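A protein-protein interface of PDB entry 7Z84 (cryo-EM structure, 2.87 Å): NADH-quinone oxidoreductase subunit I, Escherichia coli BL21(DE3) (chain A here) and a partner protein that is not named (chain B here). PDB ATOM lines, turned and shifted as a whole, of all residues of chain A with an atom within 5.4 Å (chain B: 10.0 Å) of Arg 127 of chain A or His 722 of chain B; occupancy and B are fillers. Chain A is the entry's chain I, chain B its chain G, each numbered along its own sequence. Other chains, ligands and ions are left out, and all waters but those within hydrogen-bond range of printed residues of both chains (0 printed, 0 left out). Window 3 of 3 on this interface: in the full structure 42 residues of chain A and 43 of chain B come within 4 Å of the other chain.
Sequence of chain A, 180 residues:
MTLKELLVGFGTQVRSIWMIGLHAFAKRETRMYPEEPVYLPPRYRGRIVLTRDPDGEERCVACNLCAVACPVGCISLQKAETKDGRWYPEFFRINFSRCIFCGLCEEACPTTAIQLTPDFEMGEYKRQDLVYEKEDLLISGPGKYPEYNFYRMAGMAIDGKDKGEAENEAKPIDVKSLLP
The backbone carbonyl oxygen of Thr 713 of chain B is in hydrogen-bond range of the side-chain amide nitrogen of Asn 95 of chain A (3.0 Å). The side-chain amide nitrogen (NE2) of Gln 128 of chain A lies within hydrogen-bond range of the backbone carbonyl oxygen (O) of Ala 717 of chain B (2.7 Å). O of Val 721 of chain B sits at hydrogen-bond distance from NH2 of Arg 127 of chain A (3.0 Å). The backbone NH of Val 721 of chain B sits at hydrogen-bond distance from the side-chain amide oxygen of Gln 128 of chain A (2.6 Å).
The guanidinium group (NH2) of Arg 716 of chain B is in hydrogen-bond range of the side-chain hydroxyl (OG) of Ser 720 of chain B. OG of Ser 720 of chain B sits at hydrogen-bond distance from O of His 722 of chain B (3.1 Å). The side-chain amide oxygen (OD1) of Asn 95 of chain A sits at hydrogen-bond distance from the side-chain hydroxyl (OG) of Ser 97 of chain A, at 2.9 Å.
Among the printed residues, merely in contact across the chains: Asn 95 of chain A with Val 721 of chain B, Asn 95 of chain A with Glu 723 of chain B, Ser 97 of chain A with Val 721 of chain B, Arg 127 of chain A with His 722 of chain B, Gln 128 of chain A with Asn 718 of chain B, Gln 128 of chain A with Ser 720 of chain B, Val 131 of chain A with Ala 717 of chain B and Val 131 of chain A with Val 721 of chain B.
Tyr 125 of chain A touches none of the printed residues of chain B. Arg 127 of chain A touches just these residues of chain B: Val 721 and His 722. Gln 128 of chain A touches four residues of chain B. Ala 714 of chain B touches none of the printed residues of chain A. Of the printed residues of chain A, Asn 718 of chain B touches Gln 128 (3.7 Å). Of the printed residues of chain A, Val 721 of chain B touches Asn 95 (3.4 Å), Ser 97 (3.9 Å), Arg 127 (3.0 Å), Gln 128 (2.6 Å) and Val 131 (3.8 Å).
Hydrophobic or aromatic side chains of chain B that line the printed part of chain A: Ala 717, Val 721 and His 722. Of the 9 printed residues of chain A, 5 touch a printed residue of chain B. Hydrophobic or aromatic side chains of chain A that line the printed part of chain B: Val 131. Among the printed residues, no Asp or Glu carboxylate lies within 4 Å of a Lys or Arg side-chain nitrogen of the other chain.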
ATOM      1  N   ASN A  95     -23.147  19.864  13.027  1.00  0.00           N
ATOM      2  CA  ASN A  95     -22.564  20.955  12.249  1.00  0.00           C
ATOM      3  C   ASN A  95     -23.080  20.828  10.822  1.00  0.00           C
ATOM      4  O   ASN A  95     -22.504  20.128   9.989  1.00  0.00           O
ATOM      5  CB  ASN A  95     -21.043  20.903  12.308  1.00  0.00           C
ATOM      6  CG  ASN A  95     -20.393  22.161  11.771  1.00  0.00           C
ATOM      7  OD1 ASN A  95     -21.068  23.143  11.467  1.00  0.00           O
ATOM      8  ND2 ASN A  95     -19.074  22.139  11.650  1.00  0.00           N
ATOM      9  N   SER A  97     -23.064  22.917   8.451  1.00  0.00           N
ATOM     10  CA  SER A  97     -22.147  23.414   7.436  1.00  0.00           C
ATOM     11  C   SER A  97     -21.202  22.327   6.948  1.00  0.00           C
ATOM     12  O   SER A  97     -20.645  22.452   5.853  1.00  0.00           O
ATOM     13  CB  SER A  97     -21.348  24.596   7.979  1.00  0.00           C
ATOM     14  OG  SER A  97     -20.302  24.156   8.825  1.00  0.00           O
ATOM     15  N   TYR A 125     -27.266  32.908   7.128  1.00  0.00           N
ATOM     16  CA  TYR A 125     -26.446  34.100   6.952  1.00  0.00           C
ATOM     17  C   TYR A 125     -25.082  33.972   7.618  1.00  0.00           C
ATOM     18  O   TYR A 125     -24.080  34.443   7.070  1.00  0.00           O
ATOM     19  CB  TYR A 125     -27.176  35.326   7.503  1.00  0.00           C
ATOM     20  CG  TYR A 125     -28.424  35.686   6.739  1.00  0.00           C
ATOM     21  CD1 TYR A 125     -28.363  36.021   5.394  1.00  0.00           C
ATOM     22  CD2 TYR A 125     -29.664  35.684   7.360  1.00  0.00           C
ATOM     23  CE1 TYR A 125     -29.502  36.350   4.690  1.00  0.00           C
ATOM     24  CE2 TYR A 125     -30.808  36.009   6.665  1.00  0.00           C
ATOM     25  CZ  TYR A 125     -30.722  36.343   5.330  1.00  0.00           C
ATOM     26  OH  TYR A 125     -31.859  36.669   4.629  1.00  0.00           O
ATOM     27  N   LYS A 126     -25.022  33.347   8.790  1.00  0.00           N
ATOM     28  CA  LYS A 126     -23.780  33.144   9.519  1.00  0.00           C
ATOM     29  C   LYS A 126     -23.534  31.653   9.693  1.00  0.00           C
ATOM     30  O   LYS A 126     -24.477  30.880   9.888  1.00  0.00           O
ATOM     31  CB  LYS A 126     -23.816  33.829  10.887  1.00  0.00           C
ATOM     32  CG  LYS A 126     -24.547  35.157  10.902  1.00  0.00           C
ATOM     33  CD  LYS A 126     -24.029  36.052  12.009  1.00  0.00           C
ATOM     34  CE  LYS A 126     -22.898  36.933  11.516  1.00  0.00           C
ATOM     35  NZ  LYS A 126     -23.191  37.500  10.173  1.00  0.00           N
ATOM     36  N   ARG A 127     -22.265  31.252   9.616  1.00  0.00           N
ATOM     37  CA  ARG A 127     -21.929  29.837   9.716  1.00  0.00           C
ATOM     38  C   ARG A 127     -22.070  29.300  11.133  1.00  0.00           C
ATOM     39  O   ARG A 127     -22.231  28.087  11.305  1.00  0.00           O
ATOM     40  CB  ARG A 127     -20.508  29.596   9.211  1.00  0.00           C
ATOM     41  CG  ARG A 127     -20.388  28.429   8.253  1.00  0.00           C
ATOM     42  CD  ARG A 127     -18.951  28.227   7.833  1.00  0.00           C
ATOM     43  NE  ARG A 127     -18.272  27.220   8.637  1.00  0.00           N
ATOM     44  CZ  ARG A 127     -16.955  27.085   8.709  1.00  0.00           C
ATOM     45  NH1 ARG A 127     -16.142  27.886   8.042  1.00  0.00           N
ATOM     46  NH2 ARG A 127     -16.441  26.124   9.469  1.00  0.00           N
ATOM     47  N   GLN A 128     -22.005  30.166  12.146  1.00  0.00           N
ATOM     48  CA  GLN A 128     -22.201  29.713  13.518  1.00  0.00           C
ATOM     49  C   GLN A 128     -23.649  29.316  13.772  1.00  0.00           C
ATOM     50  O   GLN A 128     -23.922  28.489  14.649  1.00  0.00           O
ATOM     51  CB  GLN A 128     -21.760  30.803  14.497  1.00  0.00           C
ATOM     52  CG  GLN A 128     -21.591  30.330  15.929  1.00  0.00           C
ATOM     53  CD  GLN A 128     -20.634  29.163  16.044  1.00  0.00           C
ATOM     54  OE1 GLN A 128     -19.512  29.214  15.545  1.00  0.00           O
ATOM     55  NE2 GLN A 128     -21.077  28.100  16.703  1.00  0.00           N
ATOM     56  N   ASP A 129     -24.583  29.874  13.006  1.00  0.00           N
ATOM     57  CA  ASP A 129     -25.991  29.525  13.128  1.00  0.00           C
ATOM     58  C   ASP A 129     -26.345  28.240  12.393  1.00  0.00           C
ATOM     59  O   ASP A 129     -27.502  27.814  12.445  1.00  0.00           O
ATOM     60  CB  ASP A 129     -26.861  30.673  12.616  1.00  0.00           C
ATOM     61  CG  ASP A 129     -26.659  31.950  13.403  1.00  0.00           C
ATOM     62  OD1 ASP A 129     -26.797  33.040  12.811  1.00  0.00           O
ATOM     63  OD2 ASP A 129     -26.363  31.865  14.613  1.00  0.00           O
ATOM     64  N   LEU A 130     -25.387  27.624  11.706  1.00  0.00           N
ATOM     65  CA  LEU A 130     -25.589  26.327  11.079  1.00  0.00           C
ATOM     66  C   LEU A 130     -25.269  25.170  12.014  1.00  0.00           C
ATOM     67  O   LEU A 130     -25.348  24.014  11.594  1.00  0.00           O
ATOM     68  CB  LEU A 130     -24.744  26.210   9.807  1.00  0.00           C
ATOM     69  CG  LEU A 130     -25.384  26.771   8.537  1.00  0.00           C
ATOM     70  CD1 LEU A 130     -24.480  26.569   7.332  1.00  0.00           C
ATOM     71  CD2 LEU A 130     -26.744  26.137   8.304  1.00  0.00           C
ATOM     72  N   VAL A 131     -24.900  25.451  13.258  1.00  0.00           N
ATOM     73  CA  VAL A 131     -24.700  24.416  14.265  1.00  0.00           C
ATOM     74  C   VAL A 131     -26.019  24.254  15.010  1.00  0.00           C
ATOM     75  O   VAL A 131     -26.389  25.098  15.830  1.00  0.00           O
ATOM     76  CB  VAL A 131     -23.553  24.768  15.218  1.00  0.00           C
ATOM     77  CG1 VAL A 131     -23.380  23.680  16.262  1.00  0.00           C
ATOM     78  CG2 VAL A 131     -22.266  24.976  14.441  1.00  0.00           C
ATOM     79  N   TYR B 638      -7.294  22.972  24.563  1.00  0.00           N
ATOM     80  CA  TYR B 638      -8.000  22.690  23.317  1.00  0.00           C
ATOM     81  C   TYR B 638      -9.440  23.181  23.378  1.00  0.00           C
ATOM     82  O   TYR B 638      -9.924  23.830  22.445  1.00  0.00           O
ATOM     83  CB  TYR B 638      -7.957  21.192  23.014  1.00  0.00           C
ATOM     84  CG  TYR B 638      -8.708  20.805  21.760  1.00  0.00           C
ATOM     85  CD1 TYR B 638      -8.194  21.096  20.503  1.00  0.00           C
ATOM     86  CD2 TYR B 638      -9.931  20.151  21.833  1.00  0.00           C
ATOM     87  CE1 TYR B 638      -8.877  20.746  19.353  1.00  0.00           C
ATOM     88  CE2 TYR B 638     -10.622  19.798  20.689  1.00  0.00           C
ATOM     89  CZ  TYR B 638     -10.090  20.097  19.452  1.00  0.00           C
ATOM     90  OH  TYR B 638     -10.774  19.747  18.311  1.00  0.00           O
ATOM     91  N   ARG B 712     -15.013  15.171  15.028  1.00  0.00           N
ATOM     92  CA  ARG B 712     -13.895  16.104  14.888  1.00  0.00           C
ATOM     93  C   ARG B 712     -14.343  17.476  14.394  1.00  0.00           C
ATOM     94  O   ARG B 712     -13.790  18.500  14.815  1.00  0.00           O
ATOM     95  CB  ARG B 712     -12.843  15.499  13.953  1.00  0.00           C
ATOM     96  CG  ARG B 712     -11.790  16.464  13.430  1.00  0.00           C
ATOM     97  CD  ARG B 712     -10.716  16.740  14.470  1.00  0.00           C
ATOM     98  NE  ARG B 712      -9.820  15.607  14.665  1.00  0.00           N
ATOM     99  CZ  ARG B 712      -8.701  15.411  13.981  1.00  0.00           C
ATOM    100  NH1 ARG B 712      -8.319  16.245  13.029  1.00  0.00           N
ATOM    101  NH2 ARG B 712      -7.944  14.354  14.263  1.00  0.00           N
ATOM    102  N   THR B 713     -15.376  17.526  13.558  1.00  0.00           N
ATOM    103  CA  THR B 713     -15.927  18.786  13.087  1.00  0.00           C
ATOM    104  C   THR B 713     -17.147  19.228  13.892  1.00  0.00           C
ATOM    105  O   THR B 713     -17.867  20.134  13.462  1.00  0.00           O
ATOM    106  CB  THR B 713     -16.270  18.682  11.603  1.00  0.00           C
ATOM    107  OG1 THR B 713     -17.238  17.647  11.405  1.00  0.00           O
ATOM    108  CG2 THR B 713     -15.023  18.340  10.815  1.00  0.00           C
ATOM    109  N   ALA B 714     -17.399  18.603  15.045  1.00  0.00           N
ATOM    110  CA  ALA B 714     -18.513  19.012  15.893  1.00  0.00           C
ATOM    111  C   ALA B 714     -18.206  19.073  17.383  1.00  0.00           C
ATOM    112  O   ALA B 714     -19.069  19.533  18.135  1.00  0.00           O
ATOM    113  CB  ALA B 714     -19.711  18.080  15.684  1.00  0.00           C
ATOM    114  N   MET B 715     -17.035  18.622  17.844  1.00  0.00           N
ATOM    115  CA  MET B 715     -16.719  18.670  19.270  1.00  0.00           C
ATOM    116  C   MET B 715     -16.606  20.097  19.788  1.00  0.00           C
ATOM    117  O   MET B 715     -16.967  20.367  20.938  1.00  0.00           O
ATOM    118  CB  MET B 715     -15.426  17.902  19.547  1.00  0.00           C
ATOM    119  CG  MET B 715     -15.558  16.398  19.417  1.00  0.00           C
ATOM    120  SD  MET B 715     -14.002  15.544  19.108  1.00  0.00           S
ATOM    121  CE  MET B 715     -12.854  16.541  20.040  1.00  0.00           C
ATOM    122  N   ARG B 716     -16.114  21.021  18.963  1.00  0.00           N
ATOM    123  CA  ARG B 716     -15.935  22.407  19.375  1.00  0.00           C
ATOM    124  C   ARG B 716     -16.845  23.361  18.611  1.00  0.00           C
ATOM    125  O   ARG B 716     -16.599  24.570  18.607  1.00  0.00           O
ATOM    126  CB  ARG B 716     -14.476  22.825  19.203  1.00  0.00           C
ATOM    127  CG  ARG B 716     -13.667  22.734  20.472  1.00  0.00           C
ATOM    128  CD  ARG B 716     -12.317  23.389  20.302  1.00  0.00           C
ATOM    129  NE  ARG B 716     -12.400  24.641  19.560  1.00  0.00           N
ATOM    130  CZ  ARG B 716     -12.210  25.837  20.097  1.00  0.00           C
ATOM    131  NH1 ARG B 716     -11.928  25.980  21.380  1.00  0.00           N
ATOM    132  NH2 ARG B 716     -12.301  26.916  19.326  1.00  0.00           N
ATOM    133  N   ALA B 717     -17.895  22.843  17.970  1.00  0.00           N
ATOM    134  CA  ALA B 717     -18.720  23.661  17.090  1.00  0.00           C
ATOM    135  C   ALA B 717     -19.568  24.678  17.842  1.00  0.00           C
ATOM    136  O   ALA B 717     -19.988  25.673  17.243  1.00  0.00           O
ATOM    137  CB  ALA B 717     -19.619  22.767  16.238  1.00  0.00           C
ATOM    138  N   ASN B 718     -19.830  24.461  19.133  1.00  0.00           N
ATOM    139  CA  ASN B 718     -20.576  25.455  19.898  1.00  0.00           C
ATOM    140  C   ASN B 718     -19.702  26.657  20.238  1.00  0.00           C
ATOM    141  O   ASN B 718     -20.186  27.794  20.268  1.00  0.00           O
ATOM    142  CB  ASN B 718     -21.150  24.829  21.169  1.00  0.00           C
ATOM    143  CG  ASN B 718     -20.091  24.179  22.032  1.00  0.00           C
ATOM    144  OD1 ASN B 718     -19.171  23.538  21.527  1.00  0.00           O
ATOM    145  ND2 ASN B 718     -20.213  24.347  23.341  1.00  0.00           N
ATOM    146  N   ILE B 719     -18.417  26.423  20.513  1.00  0.00           N
ATOM    147  CA  ILE B 719     -17.497  27.527  20.768  1.00  0.00           C
ATOM    148  C   ILE B 719     -17.239  28.310  19.486  1.00  0.00           C
ATOM    149  O   ILE B 719     -17.339  29.541  19.458  1.00  0.00           O
ATOM    150  CB  ILE B 719     -16.189  26.999  21.385  1.00  0.00           C
ATOM    151  CG1 ILE B 719     -16.427  26.535  22.821  1.00  0.00           C
ATOM    152  CG2 ILE B 719     -15.107  28.065  21.354  1.00  0.00           C
ATOM    153  CD1 ILE B 719     -16.262  25.047  23.017  1.00  0.00           C
ATOM    154  N   SER B 720     -16.930  27.602  18.403  1.00  0.00           N
ATOM    155  CA  SER B 720     -16.671  28.225  17.114  1.00  0.00           C
ATOM    156  C   SER B 720     -16.870  27.184  16.024  1.00  0.00           C
ATOM    157  O   SER B 720     -16.423  26.043  16.162  1.00  0.00           O
ATOM    158  CB  SER B 720     -15.253  28.801  17.042  1.00  0.00           C
ATOM    159  OG  SER B 720     -14.291  27.768  16.946  1.00  0.00           O
ATOM    160  N   VAL B 721     -17.534  27.586  14.939  1.00  0.00           N
ATOM    161  CA  VAL B 721     -17.770  26.669  13.832  1.00  0.00           C
ATOM    162  C   VAL B 721     -16.481  26.369  13.072  1.00  0.00           C
ATOM    163  O   VAL B 721     -16.396  25.347  12.379  1.00  0.00           O
ATOM    164  CB  VAL B 721     -18.873  27.242  12.914  1.00  0.00           C
ATOM    165  CG1 VAL B 721     -18.343  28.383  12.055  1.00  0.00           C
ATOM    166  CG2 VAL B 721     -19.503  26.148  12.063  1.00  0.00           C
ATOM    167  N   HIS B 722     -15.463  27.215  13.203  1.00  0.00           N
ATOM    168  CA  HIS B 722     -14.173  26.959  12.581  1.00  0.00           C
ATOM    169  C   HIS B 722     -13.423  25.893  13.368  1.00  0.00           C
ATOM    170  O   HIS B 722     -13.327  25.968  14.596  1.00  0.00           O
ATOM    171  CB  HIS B 722     -13.350  28.245  12.515  1.00  0.00           C
ATOM    172  CG  HIS B 722     -13.985  29.326  11.700  1.00  0.00           C
ATOM    173  ND1 HIS B 722     -13.751  29.477  10.350  1.00  0.00           N
ATOM    174  CD2 HIS B 722     -14.849  30.309  12.044  1.00  0.00           C
ATOM    175  CE1 HIS B 722     -14.442  30.508   9.898  1.00  0.00           C
ATOM    176  NE2 HIS B 722     -15.118  31.030  10.906  1.00  0.00           N
ATOM    177  N   GLU B 723     -12.896  24.904  12.662  1.00  0.00           N
ATOM    178  CA  GLU B 723     -12.148  23.843  13.323  1.00  0.00           C
ATOM    179  C   GLU B 723     -10.784  24.369  13.753  1.00  0.00           C
ATOM    180  O   GLU B 723     -10.056  24.936  12.929  1.00  0.00           O
ATOM    181  CB  GLU B 723     -11.989  22.637  12.400  1.00  0.00           C
ATOM    182  CG  GLU B 723     -13.269  21.843  12.194  1.00  0.00           C
ATOM    183  CD  GLU B 723     -14.140  22.415  11.094  1.00  0.00           C
ATOM    184  OE1 GLU B 723     -13.612  23.167  10.249  1.00  0.00           O
ATOM    185  OE2 GLU B 723     -15.352  22.116  11.075  1.00  0.00           O
ATOM    186  N   PRO B 724     -10.405  24.213  15.016  1.00  0.00           N
ATOM    187  CA  PRO B 724      -9.131  24.758  15.488  1.00  0.00           C
ATOM    188  C   PRO B 724      -7.948  23.918  15.023  1.00  0.00           C
ATOM    189  O   PRO B 724      -8.092  22.855  14.418  1.00  0.00           O
ATOM    190  CB  PRO B 724      -9.272  24.706  17.011  1.00  0.00           C
ATOM    191  CG  PRO B 724     -10.184  23.554  17.244  1.00  0.00           C
ATOM    192  CD  PRO B 724     -11.159  23.558  16.100  1.00  0.00           C
ATOM    193  N   ARG B 725      -6.759  24.439  15.310  1.00  0.00           N
ATOM    194  CA  ARG B 725      -5.526  23.716  15.040  1.00  0.00           C
ATOM    195  C   ARG B 725      -5.445  22.505  15.963  1.00  0.00           C
ATOM    196  O   ARG B 725      -5.778  22.592  17.149  1.00  0.00           O
ATOM    197  CB  ARG B 725      -4.327  24.645  15.261  1.00  0.00           C
ATOM    198  CG  ARG B 725      -2.934  24.119  14.880  1.00  0.00           C
ATOM    199  CD  ARG B 725      -2.944  23.183  13.672  1.00  0.00           C
ATOM    200  NE  ARG B 725      -1.757  22.338  13.568  1.00  0.00           N
ATOM    201  CZ  ARG B 725      -0.535  22.764  13.267  1.00  0.00           C
ATOM    202  NH1 ARG B 725      -0.288  24.034  12.988  1.00  0.00           N
ATOM    203  NH2 ARG B 725       0.464  21.887  13.222  1.00  0.00           N
ATOM    204  N   GLN B 726      -5.032  21.370  15.408  1.00  0.00           N
ATOM    205  CA  GLN B 726      -4.819  20.183  16.220  1.00  0.00           C
ATOM    206  C   GLN B 726      -3.683  20.440  17.209  1.00  0.00           C
ATOM    207  O   GLN B 726      -2.676  21.060  16.844  1.00  0.00           O
ATOM    208  CB  GLN B 726      -4.485  18.980  15.336  1.00  0.00           C
ATOM    209  CG  GLN B 726      -4.951  17.634  15.875  1.00  0.00           C
ATOM    210  CD  GLN B 726      -6.449  17.584  16.115  1.00  0.00           C
ATOM    211  OE1 GLN B 726      -7.237  18.071  15.305  1.00  0.00           O
ATOM    212  NE2 GLN B 726      -6.850  16.983  17.230  1.00  0.00           N
